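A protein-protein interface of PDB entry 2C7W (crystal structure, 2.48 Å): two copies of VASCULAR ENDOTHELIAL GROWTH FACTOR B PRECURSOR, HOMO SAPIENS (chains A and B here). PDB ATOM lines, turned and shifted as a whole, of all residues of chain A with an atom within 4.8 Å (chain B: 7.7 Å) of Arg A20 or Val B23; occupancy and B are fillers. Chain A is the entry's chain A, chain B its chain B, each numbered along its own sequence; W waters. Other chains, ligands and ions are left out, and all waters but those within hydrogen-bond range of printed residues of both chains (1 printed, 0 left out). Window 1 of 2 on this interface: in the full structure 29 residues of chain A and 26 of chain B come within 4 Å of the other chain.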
ATOM      1  N   ARG A  14     -15.654  19.908  11.506  1.00  0.00           N
ATOM      2  CA  ARG A  14     -15.454  18.572  12.067  1.00  0.00           C
ATOM      3  C   ARG A  14     -15.009  17.665  10.949  1.00  0.00           C
ATOM      4  O   ARG A  14     -14.248  16.717  11.161  1.00  0.00           O
ATOM      5  CB  ARG A  14     -16.744  17.991  12.664  1.00  0.00           C
ATOM      6  CG  ARG A  14     -17.304  18.699  13.892  1.00  0.00           C
ATOM      7  CD  ARG A  14     -18.597  18.001  14.356  1.00  0.00           C
ATOM      8  NE  ARG A  14     -19.469  18.872  15.152  1.00  0.00           N
ATOM      9  CZ  ARG A  14     -20.759  18.630  15.397  1.00  0.00           C
ATOM     10  NH1 ARG A  14     -21.344  17.536  14.913  1.00  0.00           N
ATOM     11  NH2 ARG A  14     -21.476  19.492  16.115  1.00  0.00           N
ATOM     12  N   ALA A  15     -15.497  17.961   9.753  1.00  0.00           N
ATOM     13  CA  ALA A  15     -15.182  17.178   8.574  1.00  0.00           C
ATOM     14  C   ALA A  15     -13.831  17.594   7.993  1.00  0.00           C
ATOM     15  O   ALA A  15     -13.209  16.850   7.234  1.00  0.00           O
ATOM     16  CB  ALA A  15     -16.285  17.353   7.531  1.00  0.00           C
ATOM     17  N   THR A  16     -13.388  18.793   8.350  1.00  0.00           N
ATOM     18  CA  THR A  16     -12.110  19.291   7.868  1.00  0.00           C
ATOM     19  C   THR A  16     -10.943  18.442   8.354  1.00  0.00           C
ATOM     20  O   THR A  16     -10.858  18.110   9.542  1.00  0.00           O
ATOM     21  CB  THR A  16     -11.840  20.726   8.321  1.00  0.00           C
ATOM     22  OG1 THR A  16     -12.789  21.607   7.714  1.00  0.00           O
ATOM     23  CG2 THR A  16     -10.431  21.145   7.893  1.00  0.00           C
ATOM     24  N   GLN A  18      -8.006  16.612   9.807  1.00  0.00           N
ATOM     25  CA  GLN A  18      -7.426  16.807  11.125  1.00  0.00           C
ATOM     26  C   GLN A  18      -7.197  15.461  11.804  1.00  0.00           C
ATOM     27  O   GLN A  18      -7.570  14.411  11.271  1.00  0.00           O
ATOM     28  CB  GLN A  18      -8.355  17.667  11.973  1.00  0.00           C
ATOM     29  CG  GLN A  18      -9.722  17.019  12.212  1.00  0.00           C
ATOM     30  CD  GLN A  18     -10.721  17.999  12.742  1.00  0.00           C
ATOM     31  OE1 GLN A  18     -10.763  18.281  13.938  1.00  0.00           O
ATOM     32  NE2 GLN A  18     -11.526  18.552  11.848  1.00  0.00           N
ATOM     33  N   PRO A  19      -6.563  15.469  12.983  1.00  0.00           N
ATOM     34  CA  PRO A  19      -6.310  14.218  13.702  1.00  0.00           C
ATOM     35  C   PRO A  19      -7.629  13.791  14.331  1.00  0.00           C
ATOM     36  O   PRO A  19      -8.345  14.634  14.873  1.00  0.00           O
ATOM     37  CB  PRO A  19      -5.298  14.622  14.779  1.00  0.00           C
ATOM     38  CG  PRO A  19      -4.789  15.987  14.337  1.00  0.00           C
ATOM     39  CD  PRO A  19      -5.992  16.610  13.712  1.00  0.00           C
ATOM     40  N   ARG A  20      -7.945  12.500  14.281  1.00  0.00           N
ATOM     41  CA  ARG A  20      -9.199  12.022  14.864  1.00  0.00           C
ATOM     42  C   ARG A  20      -9.155  10.526  15.183  1.00  0.00           C
ATOM     43  O   ARG A  20      -8.589   9.753  14.419  1.00  0.00           O
ATOM     44  CB  ARG A  20     -10.371  12.315  13.899  1.00  0.00           C
ATOM     45  CG  ARG A  20     -10.180  11.713  12.512  1.00  0.00           C
ATOM     46  CD  ARG A  20     -11.416  11.792  11.622  1.00  0.00           C
ATOM     47  NE  ARG A  20     -11.569  13.035  10.863  1.00  0.00           N
ATOM     48  CZ  ARG A  20     -12.273  14.090  11.266  1.00  0.00           C
ATOM     49  NH1 ARG A  20     -12.895  14.069  12.439  1.00  0.00           N
ATOM     50  NH2 ARG A  20     -12.377  15.159  10.486  1.00  0.00           N
ATOM     51  N   GLU A  21      -9.756  10.126  16.308  1.00  0.00           N
ATOM     52  CA  GLU A  21      -9.806   8.712  16.711  1.00  0.00           C
ATOM     53  C   GLU A  21     -10.179   7.829  15.532  1.00  0.00           C
ATOM     54  O   GLU A  21     -11.163   8.083  14.850  1.00  0.00           O
ATOM     55  CB  GLU A  21     -10.844   8.476  17.799  1.00  0.00           C
ATOM     56  CG  GLU A  21     -10.516   9.017  19.172  1.00  0.00           C
ATOM     57  CD  GLU A  21     -10.963   8.057  20.266  1.00  0.00           C
ATOM     58  OE1 GLU A  21     -11.220   8.508  21.406  1.00  0.00           O
ATOM     59  OE2 GLU A  21     -11.042   6.838  19.977  1.00  0.00           O
ATOM     60  N   VAL A  22      -9.397   6.784  15.315  1.00  0.00           N
ATOM     61  CA  VAL A  22      -9.613   5.858  14.219  1.00  0.00           C
ATOM     62  C   VAL A  22      -9.403   4.442  14.728  1.00  0.00           C
ATOM     63  O   VAL A  22      -8.458   4.170  15.473  1.00  0.00           O
ATOM     64  CB  VAL A  22      -8.618   6.137  13.077  1.00  0.00           C
ATOM     65  CG1 VAL A  22      -8.669   5.032  12.050  1.00  0.00           C
ATOM     66  CG2 VAL A  22      -8.941   7.487  12.430  1.00  0.00           C
ATOM     67  N   VAL A  45      -6.730   4.888  17.485  1.00  0.00           N
ATOM     68  CA  VAL A  45      -5.593   5.796  17.413  1.00  0.00           C
ATOM     69  C   VAL A  45      -5.845   7.045  16.590  1.00  0.00           C
ATOM     70  O   VAL A  45      -6.436   6.976  15.511  1.00  0.00           O
ATOM     71  CB  VAL A  45      -4.372   5.095  16.791  1.00  0.00           C
ATOM     72  CG1 VAL A  45      -3.999   3.879  17.620  1.00  0.00           C
ATOM     73  CG2 VAL A  45      -4.676   4.696  15.353  1.00  0.00           C
ATOM     74  N   GLN A  46      -5.375   8.188  17.085  1.00  0.00           N
ATOM     75  CA  GLN A  46      -5.523   9.431  16.337  1.00  0.00           C
ATOM     76  C   GLN A  46      -4.737   9.408  15.028  1.00  0.00           C
ATOM     77  O   GLN A  46      -3.533   9.162  15.013  1.00  0.00           O
ATOM     78  CB  GLN A  46      -5.054  10.619  17.160  1.00  0.00           C
ATOM     79  CG  GLN A  46      -6.053  11.077  18.183  1.00  0.00           C
ATOM     80  CD  GLN A  46      -6.025  12.576  18.333  1.00  0.00           C
ATOM     81  OE1 GLN A  46      -4.957  13.162  18.517  1.00  0.00           O
ATOM     82  NE2 GLN A  46      -7.194  13.214  18.252  1.00  0.00           N
ATOM     83  N   ARG A  47      -5.444   9.659  13.933  1.00  0.00           N
ATOM     84  CA  ARG A  47      -4.867   9.695  12.603  1.00  0.00           C
ATOM     85  C   ARG A  47      -5.435  10.915  11.903  1.00  0.00           C
ATOM     86  O   ARG A  47      -6.231  11.656  12.483  1.00  0.00           O
ATOM     87  CB  ARG A  47      -5.248   8.446  11.811  1.00  0.00           C
ATOM     88  CG  ARG A  47      -4.525   7.179  12.233  1.00  0.00           C
ATOM     89  CD  ARG A  47      -3.014   7.258  12.000  1.00  0.00           C
ATOM     90  NE  ARG A  47      -2.354   6.019  12.389  1.00  0.00           N
ATOM     91  CZ  ARG A  47      -2.430   4.884  11.704  1.00  0.00           C
ATOM     92  NH1 ARG A  47      -3.142   4.840  10.581  1.00  0.00           N
ATOM     93  NH2 ARG A  47      -1.808   3.788  12.141  1.00  0.00           N
ATOM     94  N   GLY A  49      -7.826  12.495   9.290  1.00  0.00           N
ATOM     95  CA  GLY A  49      -9.017  12.129   8.564  1.00  0.00           C
ATOM     96  C   GLY A  49      -9.817  13.359   8.248  1.00  0.00           C
ATOM     97  O   GLY A  49      -9.497  14.456   8.711  1.00  0.00           O
ATOM     98  N   GLY A  50     -10.876  13.162   7.477  1.00  0.00           N
ATOM     99  CA  GLY A  50     -11.720  14.269   7.098  1.00  0.00           C
ATOM    100  C   GLY A  50     -11.510  14.450   5.620  1.00  0.00           C
ATOM    101  O   GLY A  50     -11.188  13.497   4.912  1.00  0.00           O
ATOM    102  N   ARG B  20     -19.014   5.904  17.608  1.00  0.00           N
ATOM    103  CA  ARG B  20     -17.819   6.741  17.509  1.00  0.00           C
ATOM    104  C   ARG B  20     -17.829   7.586  16.244  1.00  0.00           C
ATOM    105  O   ARG B  20     -18.182   7.105  15.171  1.00  0.00           O
ATOM    106  CB  ARG B  20     -16.550   5.867  17.542  1.00  0.00           C
ATOM    107  CG  ARG B  20     -16.444   4.854  16.403  1.00  0.00           C
ATOM    108  CD  ARG B  20     -15.452   3.749  16.739  1.00  0.00           C
ATOM    109  NE  ARG B  20     -15.296   3.615  18.189  1.00  0.00           N
ATOM    110  CZ  ARG B  20     -14.802   2.540  18.798  1.00  0.00           C
ATOM    111  NH1 ARG B  20     -14.417   1.492  18.088  1.00  0.00           N
ATOM    112  NH2 ARG B  20     -14.688   2.506  20.117  1.00  0.00           N
ATOM    113  N   GLU B  21     -17.435   8.849  16.374  1.00  0.00           N
ATOM    114  CA  GLU B  21     -17.390   9.756  15.233  1.00  0.00           C
ATOM    115  C   GLU B  21     -16.649   9.107  14.065  1.00  0.00           C
ATOM    116  O   GLU B  21     -15.514   8.664  14.194  1.00  0.00           O
ATOM    117  CB  GLU B  21     -16.730  11.055  15.633  1.00  0.00           C
ATOM    118  N   VAL B  22     -17.329   9.038  12.931  1.00  0.00           N
ATOM    119  CA  VAL B  22     -16.800   8.432  11.720  1.00  0.00           C
ATOM    120  C   VAL B  22     -16.928   9.432  10.579  1.00  0.00           C
ATOM    121  O   VAL B  22     -17.873  10.231  10.537  1.00  0.00           O
ATOM    122  CB  VAL B  22     -17.607   7.161  11.342  1.00  0.00           C
ATOM    123  CG1 VAL B  22     -17.116   6.594  10.025  1.00  0.00           C
ATOM    124  CG2 VAL B  22     -17.496   6.119  12.457  1.00  0.00           C
ATOM    125  N   VAL B  23     -15.973   9.386   9.658  1.00  0.00           N
ATOM    126  CA  VAL B  23     -15.983  10.277   8.514  1.00  0.00           C
ATOM    127  C   VAL B  23     -16.669   9.568   7.368  1.00  0.00           C
ATOM    128  O   VAL B  23     -16.357   8.412   7.062  1.00  0.00           O
ATOM    129  CB  VAL B  23     -14.550  10.670   8.098  1.00  0.00           C
ATOM    130  CG1 VAL B  23     -14.535  11.167   6.670  1.00  0.00           C
ATOM    131  CG2 VAL B  23     -14.024  11.753   9.039  1.00  0.00           C
ATOM    132  N   VAL B  24     -17.617  10.260   6.747  1.00  0.00           N
ATOM    133  CA  VAL B  24     -18.358   9.706   5.624  1.00  0.00           C
ATOM    134  C   VAL B  24     -18.143  10.599   4.416  1.00  0.00           C
ATOM    135  O   VAL B  24     -18.425  11.800   4.456  1.00  0.00           O
ATOM    136  CB  VAL B  24     -19.874   9.617   5.924  1.00  0.00           C
ATOM    137  CG1 VAL B  24     -20.622   9.172   4.677  1.00  0.00           C
ATOM    138  CG2 VAL B  24     -20.129   8.629   7.055  1.00  0.00           C
ATOM    139  N   PRO B  25     -17.626  10.018   3.326  1.00  0.00           N
ATOM    140  CA  PRO B  25     -17.341  10.702   2.063  1.00  0.00           C
ATOM    141  C   PRO B  25     -18.607  10.960   1.270  1.00  0.00           C
ATOM    142  O   PRO B  25     -19.286  10.020   0.865  1.00  0.00           O
ATOM    143  CB  PRO B  25     -16.428   9.723   1.328  1.00  0.00           C
ATOM    144  CG  PRO B  25     -15.884   8.840   2.418  1.00  0.00           C
ATOM    145  CD  PRO B  25     -17.072   8.657   3.305  1.00  0.00           C
ATOM    146  N   LEU B  26     -18.924  12.230   1.046  1.00  0.00           N
ATOM    147  CA  LEU B  26     -20.108  12.578   0.272  1.00  0.00           C
ATOM    148  C   LEU B  26     -19.778  12.351  -1.190  1.00  0.00           C
ATOM    149  O   LEU B  26     -18.614  12.401  -1.574  1.00  0.00           O
ATOM    150  CB  LEU B  26     -20.485  14.041   0.494  1.00  0.00           C
ATOM    151  CG  LEU B  26     -20.851  14.401   1.931  1.00  0.00           C
ATOM    152  CD1 LEU B  26     -21.377  15.818   1.972  1.00  0.00           C
ATOM    153  CD2 LEU B  26     -21.892  13.428   2.454  1.00  0.00           C
ATOM    154  N   SER B  41     -17.016  18.059   1.396  1.00  0.00           N
ATOM    155  CA  SER B  41     -17.362  16.895   0.585  1.00  0.00           C
ATOM    156  C   SER B  41     -17.366  15.613   1.408  1.00  0.00           C
ATOM    157  O   SER B  41     -17.257  14.508   0.877  1.00  0.00           O
ATOM    158  CB  SER B  41     -16.406  16.748  -0.605  1.00  0.00           C
ATOM    159  OG  SER B  41     -15.093  16.423  -0.187  1.00  0.00           O
ATOM    160  N   CYS B  42     -17.498  15.767   2.717  1.00  0.00           N
ATOM    161  CA  CYS B  42     -17.553  14.619   3.599  1.00  0.00           C
ATOM    162  C   CYS B  42     -18.098  15.140   4.914  1.00  0.00           C
ATOM    163  O   CYS B  42     -18.105  16.352   5.140  1.00  0.00           O
ATOM    164  CB  CYS B  42     -16.154  14.003   3.784  1.00  0.00           C
ATOM    165  SG  CYS B  42     -15.013  14.876   4.912  1.00  0.00           S
ATOM    166  N   VAL B  43     -18.579  14.246   5.773  1.00  0.00           N
ATOM    167  CA  VAL B  43     -19.123  14.687   7.057  1.00  0.00           C
ATOM    168  C   VAL B  43     -18.709  13.726   8.159  1.00  0.00           C
ATOM    169  O   VAL B  43     -18.272  12.616   7.880  1.00  0.00           O
ATOM    170  CB  VAL B  43     -20.682  14.769   7.017  1.00  0.00           C
ATOM    171  CG1 VAL B  43     -21.129  15.709   5.909  1.00  0.00           C
ATOM    172  CG2 VAL B  43     -21.274  13.386   6.783  1.00  0.00           C
ATOM    173  N   THR B  44     -18.853  14.157   9.407  1.00  0.00           N
ATOM    174  CA  THR B  44     -18.500  13.328  10.548  1.00  0.00           C
ATOM    175  C   THR B  44     -19.793  12.926  11.251  1.00  0.00           C
ATOM    176  O   THR B  44     -20.577  13.784  11.668  1.00  0.00           O
ATOM    177  CB  THR B  44     -17.604  14.105  11.564  1.00  0.00           C
ATOM    178  OG1 THR B  44     -16.559  14.794  10.870  1.00  0.00           O
ATOM    179  CG2 THR B  44     -16.965  13.138  12.555  1.00  0.00           C
ATOM    180  N   VAL B  45     -20.009  11.623  11.403  1.00  0.00           N
ATOM    181  CA  VAL B  45     -21.223  11.134  12.047  1.00  0.00           C
ATOM    182  C   VAL B  45     -20.964   9.939  12.968  1.00  0.00           C
ATOM    183  O   VAL B  45     -20.163   9.071  12.637  1.00  0.00           O
ATOM    184  CB  VAL B  45     -22.261  10.731  10.963  1.00  0.00           C
ATOM    185  CG1 VAL B  45     -21.761   9.521  10.189  1.00  0.00           C
ATOM    186  CG2 VAL B  45     -23.630  10.471  11.602  1.00  0.00           C
ATOM    187  N   GLN B  46     -21.628   9.898  14.128  1.00  0.00           N
ATOM    188  CA  GLN B  46     -21.470   8.761  15.047  1.00  0.00           C
ATOM    189  C   GLN B  46     -21.981   7.471  14.416  1.00  0.00           C
ATOM    190  O   GLN B  46     -23.022   7.453  13.770  1.00  0.00           O
ATOM    191  CB  GLN B  46     -22.264   8.939  16.323  1.00  0.00           C
ATOM    192  CG  GLN B  46     -21.705   9.861  17.354  1.00  0.00           C
ATOM    193  CD  GLN B  46     -22.376   9.603  18.685  1.00  0.00           C
ATOM    194  OE1 GLN B  46     -23.586   9.336  18.743  1.00  0.00           O
ATOM    195  NE2 GLN B  46     -21.603   9.670  19.765  1.00  0.00           N
ATOM    196  N   ARG B  47     -21.245   6.393  14.624  1.00  0.00           N
ATOM    197  CA  ARG B  47     -21.606   5.092  14.097  1.00  0.00           C
ATOM    198  C   ARG B  47     -21.066   4.088  15.074  1.00  0.00           C
ATOM    199  O   ARG B  47     -20.372   4.460  16.023  1.00  0.00           O
ATOM    200  CB  ARG B  47     -20.962   4.854  12.735  1.00  0.00           C
ATOM    201  CG  ARG B  47     -21.565   5.679  11.620  1.00  0.00           C
ATOM    202  CD  ARG B  47     -23.057   5.417  11.509  1.00  0.00           C
ATOM    203  NE  ARG B  47     -23.674   6.240  10.488  1.00  0.00           N
ATOM    204  CZ  ARG B  47     -23.580   6.002   9.189  1.00  0.00           C
ATOM    205  NH1 ARG B  47     -22.889   4.952   8.772  1.00  0.00           N
ATOM    206  NH2 ARG B  47     -24.172   6.813   8.313  1.00  0.00           N
HETATM  207  O   HOH W   1     -18.717  16.713  10.017  1.00  0.00           O
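Water W1 bridges N of Thr B44 (2.6 Å) and N of Ala A15 (3.5 Å).
6 positions are printed for both chains. Of the 7 pairs that touch across the chains among the printed residues, none has its exchanged pair printed and touching as well.
The backbone carbonyl oxygen (O) of Arg A14 lies within hydrogen-bond range of the side-chain amide nitrogen (NE2) of Gln A18 (3.4 Å). O of Arg A47 lies within hydrogen-bond range of N of Arg A20. The backbone carbonyl oxygen of Arg A14 is in hydrogen-bond range of the guanidinium group of Arg A20 (2.5 Å). The guanidinium group (NH2) of Arg A20 lies within hydrogen-bond range of the backbone carbonyl oxygen (O) of Thr A16 (3.5 Å). The backbone NH of Val B24 lies within hydrogen-bond range of the backbone carbonyl oxygen of Val B43. O of Gly A49 sits close to NE of Arg A20 (3.3 Å).
Among the printed residues, pairs that only touch across the chains: Arg A20 with Val B23, Ala A15 with Thr B44, Gly A50 with Cys B42, Gly A50 with Val B23 and Ala A15 with Val B43.
The side-chain hydroxyl (OG1) of Thr B44 sits at hydrogen-bond distance from the backbone carbonyl oxygen (O) of Arg A14 (3.0 Å). O of Ala A15 lies close to SG of Cys B42 (3.5 Å).
Printed residues of chain A that touch a printed residue of chain B: Arg A14, Ala A15, Arg A20 and Gly A50. Hydrophobic or aromatic side chains of chain A that line the printed part of chain B: Ala A15. Of the 14 printed residues of chain B, 4 touch a printed residue of chain A. Hydrophobic or aromatic side chains of chain B within 4 Å of the printed part of chain A: Val B23. Along chain B the printed residues that touch a printed residue of chain A span positions 23 to 44. Among the printed residues, 7 pairs touch across the chains. Among the printed residues, no Asp or Glu carboxylate lies within 4 Å of a Lys or Arg side-chain nitrogen of the other chain.
Arg A20 touches just one residue of chain B: Val B23. Gly A49 touches none of the printed residues of chain B. Printed residues of chain B within 4 Å of Gly A50: Val B23 (3.8 Å) and Cys B42 (3.6 Å). Val B23 touches just these residues of chain A: Arg A20 and Gly A50. Leu B26 touches none of the printed residues of chain A. Printed residues of chain A within 4 Å of Thr B44: Arg A14 (3.0 Å) and Ala A15 (3.5 Å). The nearest residue of chain A that does not touch Val B23 is Gly A49 (4.6 Å).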
